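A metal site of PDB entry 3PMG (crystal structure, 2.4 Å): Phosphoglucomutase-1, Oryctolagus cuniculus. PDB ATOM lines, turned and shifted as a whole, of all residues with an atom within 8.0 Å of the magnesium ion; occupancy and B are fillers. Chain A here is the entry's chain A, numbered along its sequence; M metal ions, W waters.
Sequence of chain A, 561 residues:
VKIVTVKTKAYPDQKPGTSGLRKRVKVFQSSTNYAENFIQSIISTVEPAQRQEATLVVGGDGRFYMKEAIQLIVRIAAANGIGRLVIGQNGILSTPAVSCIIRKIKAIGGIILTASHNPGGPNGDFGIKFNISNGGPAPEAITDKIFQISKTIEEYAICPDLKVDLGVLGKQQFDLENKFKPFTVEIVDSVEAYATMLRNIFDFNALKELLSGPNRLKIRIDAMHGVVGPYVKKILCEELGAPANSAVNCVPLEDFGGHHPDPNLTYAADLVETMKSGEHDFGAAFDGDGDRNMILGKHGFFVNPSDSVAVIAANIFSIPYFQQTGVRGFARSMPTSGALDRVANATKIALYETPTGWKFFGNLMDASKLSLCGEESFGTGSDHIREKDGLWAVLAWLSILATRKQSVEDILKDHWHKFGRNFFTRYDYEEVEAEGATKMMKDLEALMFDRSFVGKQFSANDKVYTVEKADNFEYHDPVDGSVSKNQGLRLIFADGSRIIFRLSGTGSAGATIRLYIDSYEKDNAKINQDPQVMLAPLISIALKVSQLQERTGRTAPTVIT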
ATOM      1  N   ARG A  22      36.568   0.843   8.796  1.00  0.00           N
ATOM      2  CA  ARG A  22      36.412  -0.583   8.535  1.00  0.00           C
ATOM      3  C   ARG A  22      37.555  -1.328   7.798  1.00  0.00           C
ATOM      4  O   ARG A  22      37.923  -0.976   6.684  1.00  0.00           O
ATOM      5  CB  ARG A  22      35.114  -0.654   7.815  1.00  0.00           C
ATOM      6  CG  ARG A  22      34.530  -2.046   7.748  1.00  0.00           C
ATOM      7  CD  ARG A  22      33.040  -1.797   7.723  1.00  0.00           C
ATOM      8  NE  ARG A  22      32.613  -1.138   8.963  1.00  0.00           N
ATOM      9  CZ  ARG A  22      31.332  -0.901   9.259  1.00  0.00           C
ATOM     10  NH1 ARG A  22      30.355  -1.265   8.414  1.00  0.00           N
ATOM     11  NH2 ARG A  22      31.043  -0.309  10.446  1.00  0.00           N
ATOM     12  N   ASP A  61      29.508  -5.808  18.903  1.00  0.00           N
ATOM     13  CA  ASP A  61      28.548  -6.799  18.500  1.00  0.00           C
ATOM     14  C   ASP A  61      28.919  -8.255  18.764  1.00  0.00           C
ATOM     15  O   ASP A  61      28.252  -9.178  18.337  1.00  0.00           O
ATOM     16  CB  ASP A  61      28.220  -6.556  16.999  1.00  0.00           C
ATOM     17  CG  ASP A  61      29.336  -6.794  15.952  1.00  0.00           C
ATOM     18  OD1 ASP A  61      30.361  -7.391  16.299  1.00  0.00           O
ATOM     19  OD2 ASP A  61      29.165  -6.412  14.796  1.00  0.00           O
ATOM     20  N   THR A  95      24.419  -1.281  18.819  1.00  0.00           N
ATOM     21  CA  THR A  95      24.676   0.131  18.452  1.00  0.00           C
ATOM     22  C   THR A  95      23.588   1.014  19.055  1.00  0.00           C
ATOM     23  O   THR A  95      23.920   2.090  19.538  1.00  0.00           O
ATOM     24  CB  THR A  95      24.794   0.249  16.896  1.00  0.00           C
ATOM     25  OG1 THR A  95      26.073  -0.257  16.648  1.00  0.00           O
ATOM     26  CG2 THR A  95      24.872   1.598  16.268  1.00  0.00           C
ATOM     27  N   PRO A  96      22.308   0.611  19.113  1.00  0.00           N
ATOM     28  CA  PRO A  96      21.218   1.374  19.699  1.00  0.00           C
ATOM     29  C   PRO A  96      21.497   1.501  21.211  1.00  0.00           C
ATOM     30  O   PRO A  96      21.312   2.616  21.759  1.00  0.00           O
ATOM     31  CB  PRO A  96      19.982   0.599  19.463  1.00  0.00           C
ATOM     32  CG  PRO A  96      20.261  -0.133  18.176  1.00  0.00           C
ATOM     33  CD  PRO A  96      21.713  -0.513  18.375  1.00  0.00           C
ATOM     34  N   THR A 114      32.070  -2.909  15.700  1.00  0.00           N
ATOM     35  CA  THR A 114      31.180  -3.623  14.797  1.00  0.00           C
ATOM     36  C   THR A 114      31.533  -3.217  13.365  1.00  0.00           C
ATOM     37  O   THR A 114      32.120  -2.157  13.101  1.00  0.00           O
ATOM     38  CB  THR A 114      29.717  -3.202  15.081  1.00  0.00           C
ATOM     39  OG1 THR A 114      28.891  -3.870  14.146  1.00  0.00           O
ATOM     40  CG2 THR A 114      29.469  -1.705  14.912  1.00  0.00           C
ATOM     41  N   ALA A 115      31.212  -4.098  12.442  1.00  0.00           N
ATOM     42  CA  ALA A 115      31.377  -3.830  10.989  1.00  0.00           C
ATOM     43  C   ALA A 115      29.972  -4.168  10.487  1.00  0.00           C
ATOM     44  O   ALA A 115      29.777  -4.775   9.462  1.00  0.00           O
ATOM     45  CB  ALA A 115      32.386  -4.771  10.248  1.00  0.00           C
ATOM     46  N   SEP A 116      28.920  -3.818  11.245  1.00  0.00           N
ATOM     47  CA  SEP A 116      27.512  -4.076  10.921  1.00  0.00           C
ATOM     48  CB  SEP A 116      27.028  -2.945   9.994  1.00  0.00           C
ATOM     49  OG  SEP A 116      25.619  -2.873  10.165  1.00  0.00           O
ATOM     50  C   SEP A 116      27.160  -5.451  10.300  1.00  0.00           C
ATOM     51  O   SEP A 116      27.438  -6.481  10.896  1.00  0.00           O
ATOM     52  P   SEP A 116      24.988  -2.032   9.079  1.00  0.00           P
ATOM     53  O1P SEP A 116      25.890  -0.911   8.690  1.00  0.00           O
ATOM     54  O2P SEP A 116      23.711  -1.457   9.602  1.00  0.00           O
ATOM     55  O3P SEP A 116      24.697  -2.875   7.903  1.00  0.00           O
ATOM     56  N   HIS A 117      26.492  -5.525   9.151  1.00  0.00           N
ATOM     57  CA  HIS A 117      26.187  -6.809   8.523  1.00  0.00           C
ATOM     58  C   HIS A 117      27.426  -7.600   7.982  1.00  0.00           C
ATOM     59  O   HIS A 117      27.369  -8.738   7.506  1.00  0.00           O
ATOM     60  CB  HIS A 117      25.181  -6.535   7.397  1.00  0.00           C
ATOM     61  CG  HIS A 117      25.821  -5.796   6.215  1.00  0.00           C
ATOM     62  ND1 HIS A 117      25.883  -4.492   5.994  1.00  0.00           N
ATOM     63  CD2 HIS A 117      26.551  -6.399   5.201  1.00  0.00           C
ATOM     64  CE1 HIS A 117      26.615  -4.277   4.934  1.00  0.00           C
ATOM     65  NE2 HIS A 117      27.010  -5.437   4.470  1.00  0.00           N
ATOM     66  N   ASN A 118      28.545  -6.894   7.870  1.00  0.00           N
ATOM     67  CA  ASN A 118      29.800  -7.446   7.366  1.00  0.00           C
ATOM     68  C   ASN A 118      30.244  -8.486   8.408  1.00  0.00           C
ATOM     69  O   ASN A 118      30.446  -8.183   9.584  1.00  0.00           O
ATOM     70  CB  ASN A 118      30.934  -6.370   7.211  1.00  0.00           C
ATOM     71  CG  ASN A 118      30.569  -5.036   6.543  1.00  0.00           C
ATOM     72  OD1 ASN A 118      29.413  -4.638   6.355  1.00  0.00           O
ATOM     73  ND2 ASN A 118      31.498  -4.189   6.158  1.00  0.00           N
ATOM     74  N   LYS A 129      34.041   2.147  15.102  1.00  0.00           N
ATOM     75  CA  LYS A 129      33.184   3.313  14.896  1.00  0.00           C
ATOM     76  C   LYS A 129      33.183   4.299  16.055  1.00  0.00           C
ATOM     77  O   LYS A 129      33.092   3.892  17.211  1.00  0.00           O
ATOM     78  CB  LYS A 129      31.777   2.794  14.656  1.00  0.00           C
ATOM     79  CG  LYS A 129      30.706   3.826  14.248  1.00  0.00           C
ATOM     80  CD  LYS A 129      29.399   3.173  14.685  1.00  0.00           C
ATOM     81  CE  LYS A 129      28.168   3.730  14.030  1.00  0.00           C
ATOM     82  NZ  LYS A 129      28.207   5.169  14.111  1.00  0.00           N
ATOM     83  N   PRO A 261      25.134 -11.371   9.281  1.00  0.00           N
ATOM     84  CA  PRO A 261      23.881 -11.018   9.991  1.00  0.00           C
ATOM     85  C   PRO A 261      23.289  -9.818   9.224  1.00  0.00           C
ATOM     86  O   PRO A 261      23.478  -8.650   9.559  1.00  0.00           O
ATOM     87  CB  PRO A 261      24.353 -10.721  11.401  1.00  0.00           C
ATOM     88  CG  PRO A 261      25.716 -10.115  11.147  1.00  0.00           C
ATOM     89  CD  PRO A 261      26.334 -10.873   9.963  1.00  0.00           C
ATOM     90  N   ASP A 262      22.694 -10.092   8.057  1.00  0.00           N
ATOM     91  CA  ASP A 262      22.101  -9.042   7.247  1.00  0.00           C
ATOM     92  C   ASP A 262      20.615  -9.327   6.998  1.00  0.00           C
ATOM     93  O   ASP A 262      20.209 -10.339   6.384  1.00  0.00           O
ATOM     94  CB  ASP A 262      22.880  -8.917   5.924  1.00  0.00           C
ATOM     95  CG  ASP A 262      22.629  -7.629   5.124  1.00  0.00           C
ATOM     96  OD1 ASP A 262      22.349  -6.593   5.709  1.00  0.00           O
ATOM     97  OD2 ASP A 262      22.719  -7.651   3.906  1.00  0.00           O
ATOM     98  N   PRO A 263      19.773  -8.429   7.540  1.00  0.00           N
ATOM     99  CA  PRO A 263      18.309  -8.511   7.441  1.00  0.00           C
ATOM    100  C   PRO A 263      17.585  -8.497   6.086  1.00  0.00           C
ATOM    101  O   PRO A 263      16.960  -7.485   5.754  1.00  0.00           O
ATOM    102  CB  PRO A 263      17.881  -7.386   8.405  1.00  0.00           C
ATOM    103  CG  PRO A 263      18.922  -6.313   8.194  1.00  0.00           C
ATOM    104  CD  PRO A 263      20.179  -7.169   8.176  1.00  0.00           C
ATOM    105  N   PHE A 286      17.365  -9.217  12.290  1.00  0.00           N
ATOM    106  CA  PHE A 286      18.158  -8.023  12.485  1.00  0.00           C
ATOM    107  C   PHE A 286      19.604  -8.027  12.017  1.00  0.00           C
ATOM    108  O   PHE A 286      20.168  -9.096  11.774  1.00  0.00           O
ATOM    109  CB  PHE A 286      18.225  -7.615  13.962  1.00  0.00           C
ATOM    110  CG  PHE A 286      16.920  -7.593  14.754  1.00  0.00           C
ATOM    111  CD1 PHE A 286      16.078  -6.501  14.635  1.00  0.00           C
ATOM    112  CD2 PHE A 286      16.624  -8.689  15.599  1.00  0.00           C
ATOM    113  CE1 PHE A 286      14.912  -6.502  15.373  1.00  0.00           C
ATOM    114  CE2 PHE A 286      15.453  -8.667  16.330  1.00  0.00           C
ATOM    115  CZ  PHE A 286      14.600  -7.570  16.219  1.00  0.00           C
ATOM    116  N   ASP A 287      20.261  -6.869  11.832  1.00  0.00           N
ATOM    117  CA  ASP A 287      21.658  -6.904  11.394  1.00  0.00           C
ATOM    118  C   ASP A 287      22.688  -7.126  12.519  1.00  0.00           C
ATOM    119  O   ASP A 287      22.356  -7.081  13.722  1.00  0.00           O
ATOM    120  CB  ASP A 287      22.051  -5.612  10.616  1.00  0.00           C
ATOM    121  CG  ASP A 287      22.167  -4.305  11.355  1.00  0.00           C
ATOM    122  OD1 ASP A 287      21.365  -4.066  12.252  1.00  0.00           O
ATOM    123  OD2 ASP A 287      23.051  -3.538  11.034  1.00  0.00           O
ATOM    124  N   GLY A 288      23.965  -7.226  12.187  1.00  0.00           N
ATOM    125  CA  GLY A 288      24.963  -7.474  13.251  1.00  0.00           C
ATOM    126  C   GLY A 288      24.972  -6.700  14.572  1.00  0.00           C
ATOM    127  O   GLY A 288      25.045  -7.296  15.646  1.00  0.00           O
ATOM    128  N   ASP A 289      24.895  -5.359  14.408  1.00  0.00           N
ATOM    129  CA  ASP A 289      24.887  -4.374  15.498  1.00  0.00           C
ATOM    130  C   ASP A 289      23.519  -3.830  15.961  1.00  0.00           C
ATOM    131  O   ASP A 289      23.405  -2.779  16.564  1.00  0.00           O
ATOM    132  CB  ASP A 289      25.834  -3.230  15.043  1.00  0.00           C
ATOM    133  CG  ASP A 289      25.331  -2.306  13.912  1.00  0.00           C
ATOM    134  OD1 ASP A 289      24.560  -2.707  13.034  1.00  0.00           O
ATOM    135  OD2 ASP A 289      25.738  -1.159  13.951  1.00  0.00           O
ATOM    136  N   GLY A 290      22.434  -4.459  15.550  1.00  0.00           N
ATOM    137  CA  GLY A 290      21.043  -4.126  15.904  1.00  0.00           C
ATOM    138  C   GLY A 290      20.295  -2.915  15.324  1.00  0.00           C
ATOM    139  O   GLY A 290      19.097  -2.709  15.620  1.00  0.00           O
ATOM    140  N   ASP A 291      20.943  -2.025  14.546  1.00  0.00           N
ATOM    141  CA  ASP A 291      20.202  -0.875  13.987  1.00  0.00           C
ATOM    142  C   ASP A 291      19.371  -1.052  12.682  1.00  0.00           C
ATOM    143  O   ASP A 291      18.890  -0.087  12.088  1.00  0.00           O
ATOM    144  CB  ASP A 291      21.206   0.293  13.796  1.00  0.00           C
ATOM    145  CG  ASP A 291      22.168   0.114  12.654  1.00  0.00           C
ATOM    146  OD1 ASP A 291      22.518  -1.034  12.405  1.00  0.00           O
ATOM    147  OD2 ASP A 291      22.565   1.103  12.059  1.00  0.00           O
ATOM    148  N   ARG A 292      19.207  -2.291  12.168  1.00  0.00           N
ATOM    149  CA  ARG A 292      18.431  -2.501  10.940  1.00  0.00           C
ATOM    150  C   ARG A 292      17.519  -3.707  11.210  1.00  0.00           C
ATOM    151  O   ARG A 292      17.895  -4.524  12.082  1.00  0.00           O
ATOM    152  CB  ARG A 292      19.361  -2.791   9.763  1.00  0.00           C
ATOM    153  CG  ARG A 292      20.157  -1.554   9.330  1.00  0.00           C
ATOM    154  CD  ARG A 292      20.645  -1.614   7.897  1.00  0.00           C
ATOM    155  NE  ARG A 292      21.744  -2.542   7.818  1.00  0.00           N
ATOM    156  CZ  ARG A 292      21.731  -3.690   7.149  1.00  0.00           C
ATOM    157  NH1 ARG A 292      20.686  -4.102   6.454  1.00  0.00           N
ATOM    158  NH2 ARG A 292      22.778  -4.494   7.307  1.00  0.00           N
ATOM    159  N   ASN A 293      16.362  -3.845  10.514  1.00  0.00           N
ATOM    160  CA  ASN A 293      15.348  -4.910  10.692  1.00  0.00           C
ATOM    161  C   ASN A 293      14.545  -5.311   9.434  1.00  0.00           C
ATOM    162  O   ASN A 293      14.453  -4.542   8.500  1.00  0.00           O
ATOM    163  CB  ASN A 293      14.312  -4.476  11.723  1.00  0.00           C
ATOM    164  CG  ASN A 293      13.449  -3.258  11.320  1.00  0.00           C
ATOM    165  OD1 ASN A 293      13.874  -2.085  11.198  1.00  0.00           O
ATOM    166  ND2 ASN A 293      12.169  -3.476  11.061  1.00  0.00           N
ATOM    167  N   GLU A 387      20.719   6.858  16.273  1.00  0.00           N
ATOM    168  CA  GLU A 387      21.173   5.748  15.430  1.00  0.00           C
ATOM    169  C   GLU A 387      19.897   5.027  15.051  1.00  0.00           C
ATOM    170  O   GLU A 387      18.830   5.351  15.635  1.00  0.00           O
ATOM    171  CB  GLU A 387      22.026   4.750  16.137  1.00  0.00           C
ATOM    172  CG  GLU A 387      23.420   5.264  16.436  1.00  0.00           C
ATOM    173  CD  GLU A 387      24.456   4.972  15.382  1.00  0.00           C
ATOM    174  OE1 GLU A 387      24.088   4.608  14.275  1.00  0.00           O
ATOM    175  OE2 GLU A 387      25.630   5.040  15.668  1.00  0.00           O
ATOM    176  N   LYS A 388      19.897   4.148  14.045  1.00  0.00           N
ATOM    177  CA  LYS A 388      18.665   3.423  13.735  1.00  0.00           C
ATOM    178  C   LYS A 388      18.486   2.301  14.756  1.00  0.00           C
ATOM    179  O   LYS A 388      19.436   1.848  15.444  1.00  0.00           O
ATOM    180  CB  LYS A 388      18.705   2.811  12.380  1.00  0.00           C
ATOM    181  CG  LYS A 388      18.521   3.776  11.153  1.00  0.00           C
ATOM    182  CD  LYS A 388      19.506   3.469   9.970  1.00  0.00           C
ATOM    183  CE  LYS A 388      19.561   1.980   9.661  1.00  0.00           C
ATOM    184  NZ  LYS A 388      20.529   1.718   8.612  1.00  0.00           N
ATOM    185  N   GLY A 390      16.586  -1.512  15.046  1.00  0.00           N
ATOM    186  CA  GLY A 390      15.740  -2.560  14.529  1.00  0.00           C
ATOM    187  C   GLY A 390      14.762  -3.065  15.547  1.00  0.00           C
ATOM    188  O   GLY A 390      13.585  -3.236  15.270  1.00  0.00           O
HETATM  189 MG    MG M   1      23.758  -1.927  11.647  1.00  0.00          MG
HETATM  190  O   HOH W   1      25.023  -0.474  11.459  1.00  0.00           O
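OD1 of Asp 287 sits at hydrogen-bond distance from N of Arg 292, at 2.8 Å.
O3P of SEP 116 is in hydrogen-bond range of a ring nitrogen (ND1) of His 117 (2.8 Å).
N of SEP 116 lies within hydrogen-bond range of OG1 of Thr 114, at 2.9 Å.
NH2 of Arg 292 lies within salt-bridge range of O3P of SEP 116, at 2.6 Å.
The side-chain carboxylate of Asp 289 is in hydrogen-bond range of the side-chain hydroxyl of Thr 95, at 2.9 Å.
OD1 of Asp 287 sits close to N of Gly 290 (3.5 Å).
Within 4 Å of the magnesium ion: SEP 116, Asp 287, Asp 289 and Asp 291.
The nearest printed residue that does not touch the magnesium ion is Arg 292 (4.3 Å).
The magnesium ion is bound by the side-chain carboxylate (OD1) of Asp 291, the side-chain carboxylate (OD1) of Asp 289, the side-chain carboxylate (OD2) of Asp 287, water W1, O2P of SEP 116 and OG of SEP 116.
The magnesium ion has six donor atoms within binding distance.
Water W1 lies within hydrogen-bond range of the side-chain carboxylate (OD2) of Asp 289 (2.7 Å), O1P of SEP 116 (2.9 Å) and the side-chain carboxylate (OD2) of Asp 291 (3.0 Å).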
